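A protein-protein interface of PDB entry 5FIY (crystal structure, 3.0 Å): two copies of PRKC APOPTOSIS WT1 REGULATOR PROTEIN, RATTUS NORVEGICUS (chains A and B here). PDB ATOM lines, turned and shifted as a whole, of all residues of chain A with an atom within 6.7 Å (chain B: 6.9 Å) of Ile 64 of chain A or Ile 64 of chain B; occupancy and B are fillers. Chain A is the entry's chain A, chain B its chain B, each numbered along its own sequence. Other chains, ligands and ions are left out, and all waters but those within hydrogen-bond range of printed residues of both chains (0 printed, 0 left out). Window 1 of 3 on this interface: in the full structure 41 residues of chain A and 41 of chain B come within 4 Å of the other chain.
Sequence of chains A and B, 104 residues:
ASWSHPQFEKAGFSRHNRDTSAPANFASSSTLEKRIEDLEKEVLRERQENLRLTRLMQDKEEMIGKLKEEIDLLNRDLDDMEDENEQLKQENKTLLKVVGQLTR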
ATOM      1  N   ASP A  59      17.289  33.691  -6.198  1.00  0.00           N
ATOM      2  CA  ASP A  59      17.287  32.656  -7.232  1.00  0.00           C
ATOM      3  C   ASP A  59      15.991  31.849  -7.228  1.00  0.00           C
ATOM      4  O   ASP A  59      15.312  31.775  -8.254  1.00  0.00           O
ATOM      5  CB  ASP A  59      18.482  31.717  -7.084  1.00  0.00           C
ATOM      6  CG  ASP A  59      19.786  32.377  -7.477  1.00  0.00           C
ATOM      7  OD1 ASP A  59      19.788  33.605  -7.718  1.00  0.00           O
ATOM      8  OD2 ASP A  59      20.807  31.662  -7.568  1.00  0.00           O
ATOM      9  N   LYS A  60      15.657  31.233  -6.097  1.00  0.00           N
ATOM     10  CA  LYS A  60      14.430  30.437  -6.010  1.00  0.00           C
ATOM     11  C   LYS A  60      13.195  31.206  -6.490  1.00  0.00           C
ATOM     12  O   LYS A  60      12.340  30.636  -7.169  1.00  0.00           O
ATOM     13  CB  LYS A  60      14.208  29.940  -4.579  1.00  0.00           C
ATOM     14  CG  LYS A  60      15.360  29.117  -4.020  1.00  0.00           C
ATOM     15  CD  LYS A  60      15.782  28.004  -4.970  1.00  0.00           C
ATOM     16  CE  LYS A  60      17.032  27.293  -4.469  1.00  0.00           C
ATOM     17  NZ  LYS A  60      17.639  26.409  -5.509  1.00  0.00           N
ATOM     18  N   GLU A  61      13.100  32.487  -6.145  1.00  0.00           N
ATOM     19  CA  GLU A  61      11.965  33.300  -6.586  1.00  0.00           C
ATOM     20  C   GLU A  61      11.953  33.536  -8.094  1.00  0.00           C
ATOM     21  O   GLU A  61      10.889  33.468  -8.724  1.00  0.00           O
ATOM     22  CB  GLU A  61      11.931  34.639  -5.845  1.00  0.00           C
ATOM     23  CG  GLU A  61      11.097  34.617  -4.572  1.00  0.00           C
ATOM     24  CD  GLU A  61       9.610  34.414  -4.851  1.00  0.00           C
ATOM     25  OE1 GLU A  61       9.188  34.559  -6.019  1.00  0.00           O
ATOM     26  OE2 GLU A  61       8.860  34.111  -3.901  1.00  0.00           O
ATOM     27  N   GLU A  62      13.121  33.811  -8.675  1.00  0.00           N
ATOM     28  CA  GLU A  62      13.192  33.929 -10.132  1.00  0.00           C
ATOM     29  C   GLU A  62      12.717  32.640 -10.800  1.00  0.00           C
ATOM     30  O   GLU A  62      11.847  32.651 -11.689  1.00  0.00           O
ATOM     31  CB  GLU A  62      14.615  34.248 -10.596  1.00  0.00           C
ATOM     32  CG  GLU A  62      15.024  35.703 -10.470  1.00  0.00           C
ATOM     33  CD  GLU A  62      16.313  35.992 -11.218  1.00  0.00           C
ATOM     34  OE1 GLU A  62      16.855  35.056 -11.844  1.00  0.00           O
ATOM     35  OE2 GLU A  62      16.777  37.152 -11.192  1.00  0.00           O
ATOM     36  N   MET A  63      13.299  31.531 -10.349  1.00  0.00           N
ATOM     37  CA  MET A  63      12.936  30.200 -10.827  1.00  0.00           C
ATOM     38  C   MET A  63      11.425  29.980 -10.783  1.00  0.00           C
ATOM     39  O   MET A  63      10.817  29.583 -11.780  1.00  0.00           O
ATOM     40  CB  MET A  63      13.646  29.131  -9.995  1.00  0.00           C
ATOM     41  CG  MET A  63      13.204  27.715 -10.308  1.00  0.00           C
ATOM     42  SD  MET A  63      13.619  27.190 -12.135  1.00  0.00           S
ATOM     43  CE  MET A  63      15.560  27.403 -12.082  1.00  0.00           C
ATOM     44  N   ILE A  64      10.830  30.247  -9.624  1.00  0.00           N
ATOM     45  CA  ILE A  64       9.384  30.171  -9.458  1.00  0.00           C
ATOM     46  C   ILE A  64       8.654  31.022 -10.492  1.00  0.00           C
ATOM     47  O   ILE A  64       7.665  30.579 -11.080  1.00  0.00           O
ATOM     48  CB  ILE A  64       8.961  30.609  -8.042  1.00  0.00           C
ATOM     49  CG1 ILE A  64       9.365  29.542  -7.024  1.00  0.00           C
ATOM     50  CG2 ILE A  64       7.461  30.828  -7.973  1.00  0.00           C
ATOM     51  CD1 ILE A  64       9.155  29.956  -5.590  1.00  0.00           C
ATOM     52  N   GLY A  65       9.143  32.239 -10.717  1.00  0.00           N
ATOM     53  CA  GLY A  65       8.546  33.116 -11.709  1.00  0.00           C
ATOM     54  C   GLY A  65       8.501  32.477 -13.087  1.00  0.00           C
ATOM     55  O   GLY A  65       7.432  32.376 -13.711  1.00  0.00           O
ATOM     56  N   LYS A  66       9.662  32.030 -13.558  1.00  0.00           N
ATOM     57  CA  LYS A  66       9.739  31.354 -14.853  1.00  0.00           C
ATOM     58  C   LYS A  66       8.823  30.132 -14.932  1.00  0.00           C
ATOM     59  O   LYS A  66       8.140  29.932 -15.933  1.00  0.00           O
ATOM     60  CB  LYS A  66      11.183  30.964 -15.180  1.00  0.00           C
ATOM     61  CG  LYS A  66      12.020  32.139 -15.665  1.00  0.00           C
ATOM     62  CD  LYS A  66      13.465  31.751 -15.907  1.00  0.00           C
ATOM     63  CE  LYS A  66      14.282  32.961 -16.333  1.00  0.00           C
ATOM     64  NZ  LYS A  66      15.745  32.679 -16.395  1.00  0.00           N
ATOM     65  N   LEU A  67       8.822  29.310 -13.888  1.00  0.00           N
ATOM     66  CA  LEU A  67       7.960  28.130 -13.848  1.00  0.00           C
ATOM     67  C   LEU A  67       6.476  28.489 -13.975  1.00  0.00           C
ATOM     68  O   LEU A  67       5.731  27.841 -14.720  1.00  0.00           O
ATOM     69  CB  LEU A  67       8.198  27.353 -12.552  1.00  0.00           C
ATOM     70  CG  LEU A  67       9.583  26.725 -12.398  1.00  0.00           C
ATOM     71  CD1 LEU A  67       9.692  25.951 -11.092  1.00  0.00           C
ATOM     72  CD2 LEU A  67       9.881  25.818 -13.581  1.00  0.00           C
ATOM     73  N   LYS A  68       6.055  29.528 -13.258  1.00  0.00           N
ATOM     74  CA  LYS A  68       4.667  29.981 -13.310  1.00  0.00           C
ATOM     75  C   LYS A  68       4.316  30.487 -14.706  1.00  0.00           C
ATOM     76  O   LYS A  68       3.229  30.218 -15.224  1.00  0.00           O
ATOM     77  CB  LYS A  68       4.412  31.074 -12.269  1.00  0.00           C
ATOM     78  CG  LYS A  68       4.247  30.558 -10.847  1.00  0.00           C
ATOM     79  CD  LYS A  68       3.855  31.675  -9.891  1.00  0.00           C
ATOM     80  CE  LYS A  68       3.747  31.169  -8.461  1.00  0.00           C
ATOM     81  NZ  LYS A  68       3.573  32.287  -7.492  1.00  0.00           N
ATOM     82  N   GLU A  69       5.254  31.212 -15.309  1.00  0.00           N
ATOM     83  CA  GLU A  69       5.095  31.700 -16.677  1.00  0.00           C
ATOM     84  C   GLU A  69       4.914  30.548 -17.674  1.00  0.00           C
ATOM     85  O   GLU A  69       4.020  30.569 -18.530  1.00  0.00           O
ATOM     86  CB  GLU A  69       6.307  32.553 -17.061  1.00  0.00           C
ATOM     87  CG  GLU A  69       6.195  33.257 -18.396  1.00  0.00           C
ATOM     88  CD  GLU A  69       7.370  34.180 -18.658  1.00  0.00           C
ATOM     89  OE1 GLU A  69       7.694  35.003 -17.774  1.00  0.00           O
ATOM     90  OE2 GLU A  69       7.973  34.080 -19.748  1.00  0.00           O
ATOM     91  N   GLN B  58      13.020  26.405   2.390  1.00  0.00           N
ATOM     92  CA  GLN B  58      12.324  25.132   2.199  1.00  0.00           C
ATOM     93  C   GLN B  58      10.944  25.321   1.557  1.00  0.00           C
ATOM     94  O   GLN B  58      10.546  24.530   0.690  1.00  0.00           O
ATOM     95  CB  GLN B  58      12.191  24.369   3.517  1.00  0.00           C
ATOM     96  CG  GLN B  58      13.520  23.955   4.121  1.00  0.00           C
ATOM     97  CD  GLN B  58      13.360  23.287   5.472  1.00  0.00           C
ATOM     98  OE1 GLN B  58      12.250  22.957   5.886  1.00  0.00           O
ATOM     99  NE2 GLN B  58      14.476  23.077   6.161  1.00  0.00           N
ATOM    100  N   ASP B  59      10.221  26.362   1.972  1.00  0.00           N
ATOM    101  CA  ASP B  59       8.951  26.692   1.314  1.00  0.00           C
ATOM    102  C   ASP B  59       9.127  26.898  -0.194  1.00  0.00           C
ATOM    103  O   ASP B  59       8.475  26.221  -0.990  1.00  0.00           O
ATOM    104  CB  ASP B  59       8.306  27.925   1.945  1.00  0.00           C
ATOM    105  CG  ASP B  59       7.751  27.643   3.325  1.00  0.00           C
ATOM    106  OD1 ASP B  59       8.007  26.535   3.845  1.00  0.00           O
ATOM    107  OD2 ASP B  59       7.044  28.516   3.877  1.00  0.00           O
ATOM    108  N   LYS B  60       9.989  27.837  -0.581  1.00  0.00           N
ATOM    109  CA  LYS B  60      10.278  28.086  -1.995  1.00  0.00           C
ATOM    110  C   LYS B  60      10.637  26.797  -2.738  1.00  0.00           C
ATOM    111  O   LYS B  60      10.245  26.608  -3.890  1.00  0.00           O
ATOM    112  CB  LYS B  60      11.425  29.092  -2.162  1.00  0.00           C
ATOM    113  CG  LYS B  60      11.225  30.473  -1.548  1.00  0.00           C
ATOM    114  CD  LYS B  60       9.920  31.137  -1.958  1.00  0.00           C
ATOM    115  CE  LYS B  60       9.745  32.462  -1.217  1.00  0.00           C
ATOM    116  NZ  LYS B  60       8.374  33.037  -1.347  1.00  0.00           N
ATOM    117  N   GLU B  61      11.388  25.920  -2.078  1.00  0.00           N
ATOM    118  CA  GLU B  61      11.806  24.658  -2.686  1.00  0.00           C
ATOM    119  C   GLU B  61      10.611  23.741  -2.962  1.00  0.00           C
ATOM    120  O   GLU B  61      10.481  23.156  -4.053  1.00  0.00           O
ATOM    121  CB  GLU B  61      12.800  23.939  -1.764  1.00  0.00           C
ATOM    122  CG  GLU B  61      14.264  24.341  -1.925  1.00  0.00           C
ATOM    123  CD  GLU B  61      14.853  23.970  -3.273  1.00  0.00           C
ATOM    124  OE1 GLU B  61      14.230  23.177  -4.010  1.00  0.00           O
ATOM    125  OE2 GLU B  61      15.958  24.460  -3.586  1.00  0.00           O
ATOM    126  N   GLU B  62       9.723  23.654  -1.973  1.00  0.00           N
ATOM    127  CA  GLU B  62       8.487  22.894  -2.099  1.00  0.00           C
ATOM    128  C   GLU B  62       7.655  23.430  -3.260  1.00  0.00           C
ATOM    129  O   GLU B  62       7.109  22.668  -4.071  1.00  0.00           O
ATOM    130  CB  GLU B  62       7.689  22.958  -0.793  1.00  0.00           C
ATOM    131  CG  GLU B  62       6.458  22.062  -0.754  1.00  0.00           C
ATOM    132  CD  GLU B  62       5.742  22.121   0.584  1.00  0.00           C
ATOM    133  OE1 GLU B  62       6.165  22.920   1.448  1.00  0.00           O
ATOM    134  OE2 GLU B  62       4.761  21.370   0.773  1.00  0.00           O
ATOM    135  N   MET B  63       7.584  24.757  -3.333  1.00  0.00           N
ATOM    136  CA  MET B  63       6.847  25.437  -4.388  1.00  0.00           C
ATOM    137  C   MET B  63       7.406  25.098  -5.766  1.00  0.00           C
ATOM    138  O   MET B  63       6.650  24.792  -6.684  1.00  0.00           O
ATOM    139  CB  MET B  63       6.876  26.949  -4.166  1.00  0.00           C
ATOM    140  CG  MET B  63       6.103  27.733  -5.209  1.00  0.00           C
ATOM    141  SD  MET B  63       4.227  27.212  -5.244  1.00  0.00           S
ATOM    142  CE  MET B  63       3.459  28.693  -4.227  1.00  0.00           C
ATOM    143  N   ILE B  64       8.729  25.156  -5.903  1.00  0.00           N
ATOM    144  CA  ILE B  64       9.385  24.761  -7.145  1.00  0.00           C
ATOM    145  C   ILE B  64       9.025  23.329  -7.523  1.00  0.00           C
ATOM    146  O   ILE B  64       8.683  23.050  -8.676  1.00  0.00           O
ATOM    147  CB  ILE B  64      10.923  24.885  -7.048  1.00  0.00           C
ATOM    148  CG1 ILE B  64      11.343  26.354  -7.023  1.00  0.00           C
ATOM    149  CG2 ILE B  64      11.596  24.184  -8.217  1.00  0.00           C
ATOM    150  CD1 ILE B  64      12.817  26.550  -6.760  1.00  0.00           C
ATOM    151  N   GLY B  65       9.079  22.428  -6.546  1.00  0.00           N
ATOM    152  CA  GLY B  65       8.710  21.045  -6.799  1.00  0.00           C
ATOM    153  C   GLY B  65       7.301  20.901  -7.351  1.00  0.00           C
ATOM    154  O   GLY B  65       7.089  20.308  -8.424  1.00  0.00           O
ATOM    155  N   LYS B  66       6.334  21.467  -6.630  1.00  0.00           N
ATOM    156  CA  LYS B  66       4.938  21.437  -7.070  1.00  0.00           C
ATOM    157  C   LYS B  66       4.737  22.034  -8.464  1.00  0.00           C
ATOM    158  O   LYS B  66       4.025  21.458  -9.283  1.00  0.00           O
ATOM    159  CB  LYS B  66       4.034  22.150  -6.056  1.00  0.00           C
ATOM    160  CG  LYS B  66       3.712  21.308  -4.829  1.00  0.00           C
ATOM    161  CD  LYS B  66       2.894  22.085  -3.807  1.00  0.00           C
ATOM    162  CE  LYS B  66       2.609  21.241  -2.568  1.00  0.00           C
ATOM    163  NZ  LYS B  66       3.788  20.433  -2.137  1.00  0.00           N
ATOM    164  N   LEU B  67       5.342  23.188  -8.727  1.00  0.00           N
ATOM    165  CA  LEU B  67       5.243  23.807 -10.048  1.00  0.00           C
ATOM    166  C   LEU B  67       5.804  22.917 -11.154  1.00  0.00           C
ATOM    167  O   LEU B  67       5.211  22.810 -12.226  1.00  0.00           O
ATOM    168  CB  LEU B  67       5.953  25.162 -10.071  1.00  0.00           C
ATOM    169  CG  LEU B  67       5.347  26.270  -9.206  1.00  0.00           C
ATOM    170  CD1 LEU B  67       6.121  27.570  -9.381  1.00  0.00           C
ATOM    171  CD2 LEU B  67       3.872  26.461  -9.526  1.00  0.00           C
ATOM    172  N   LYS B  68       6.947  22.287 -10.901  1.00  0.00           N
ATOM    173  CA  LYS B  68       7.551  21.401 -11.898  1.00  0.00           C
ATOM    174  C   LYS B  68       6.646  20.198 -12.179  1.00  0.00           C
ATOM    175  O   LYS B  68       6.455  19.793 -13.340  1.00  0.00           O
ATOM    176  CB  LYS B  68       8.938  20.950 -11.433  1.00  0.00           C
ATOM    177  CG  LYS B  68       9.993  22.032 -11.610  1.00  0.00           C
ATOM    178  CD  LYS B  68      11.393  21.554 -11.274  1.00  0.00           C
ATOM    179  CE  LYS B  68      12.384  22.704 -11.414  1.00  0.00           C
ATOM    180  NZ  LYS B  68      13.740  22.360 -10.903  1.00  0.00           N
ATOM    181  N   GLU B  69       6.064  19.648 -11.113  1.00  0.00           N
ATOM    182  CA  GLU B  69       5.103  18.559 -11.264  1.00  0.00           C
ATOM    183  C   GLU B  69       3.915  18.998 -12.110  1.00  0.00           C
ATOM    184  O   GLU B  69       3.467  18.275 -13.004  1.00  0.00           O
ATOM    185  CB  GLU B  69       4.616  18.067  -9.897  1.00  0.00           C
ATOM    186  CG  GLU B  69       3.702  16.849  -9.961  1.00  0.00           C
ATOM    187  CD  GLU B  69       4.246  15.738 -10.840  1.00  0.00           C
ATOM    188  OE1 GLU B  69       5.451  15.425 -10.733  1.00  0.00           O
ATOM    189  OE2 GLU B  69       3.460  15.179 -11.639  1.00  0.00           O
ATOM    190  N   GLU B  70       3.414  20.191 -11.812  1.00  0.00           N
ATOM    191  CA  GLU B  70       2.313  20.785 -12.556  1.00  0.00           C
ATOM    192  C   GLU B  70       2.657  20.915 -14.041  1.00  0.00           C
ATOM    193  O   GLU B  70       1.821  20.660 -14.900  1.00  0.00           O
ATOM    194  CB  GLU B  70       1.954  22.151 -11.970  1.00  0.00           C
ATOM    195  CG  GLU B  70       0.779  22.817 -12.648  1.00  0.00           C
ATOM    196  CD  GLU B  70      -0.504  22.024 -12.468  1.00  0.00           C
ATOM    197  OE1 GLU B  70      -0.625  21.310 -11.448  1.00  0.00           O
ATOM    198  OE2 GLU B  70      -1.387  22.109 -13.346  1.00  0.00           O
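The side-chain carboxylate of Glu 61 of chain B is in salt-bridge range of the side-chain amino group of Lys 60 of chain A (3.2 Å). The side-chain carboxylate (OE2) of Glu 61 of chain A is in salt-bridge range of the side-chain amino group (NZ) of Lys 60 of chain B (2.8 Å).
Among the printed residues, merely in contact across the chains: Lys 60 of chain A with Lys 60 of chain B, Lys 60 of chain A with Ile 64 of chain B, Met 63 of chain A with Ile 64 of chain B, Ile 64 of chain A with Lys 60 of chain B, Ile 64 of chain A with Met 63 of chain B, Ile 64 of chain A with Ile 64 of chain B, Ile 64 of chain A with Leu 67 of chain B, Leu 67 of chain A with Ile 64 of chain B, Leu 67 of chain A with Leu 67 of chain B, Leu 67 of chain A with Lys 68 of chain B and Lys 68 of chain A with Leu 67 of chain B.
Glu 69 of chain A touches none of the printed residues of chain B. Of the printed residues of chain A, Glu 61 of chain B touches Lys 60 (3.2 Å). Of the printed residues of chain A, Met 63 of chain B touches Ile 64. Ile 64 of chain B touches four residues of chain A. Of the printed residues of chain A, Leu 67 of chain B touches Ile 64, Leu 67 and Lys 68. The nearest residue of chain B that does not touch Ile 64 of chain A is Glu 61 of chain B (5.8 Å).
Of the 13 printed residues of chain B, 6 touch a printed residue of chain A. Printed residues of chain B that touch a printed residue of chain A: Lys 60, Glu 61, Met 63, Ile 64, Leu 67 and Lys 68. Among the printed residues, 13 pairs touch across the chains. Among the printed residues, Asp or Glu carboxylates within 4 Å of a Lys or Arg side-chain nitrogen of the other chain: Lys 60 of chain A with Glu 61 of chain B and Glu 61 of chain A with Lys 60 of chain B.
Lys 60 of chain A touches Glu 61 of chain B, and with the chains exchanged Glu 61 of chain A touches Lys 60 of chain B. Ile 64 of chain A touches its own counterpart, Ile 64 of chain B. Ile 64 of chain A touches Leu 67 of chain B, and with the chains exchanged Leu 67 of chain A touches Ile 64 of chain B. Leu 67 of chain A touches Lys 68 of chain B, and with the chains exchanged Lys 68 of chain A touches Leu 67 of chain B. 11 positions are printed for both chains.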
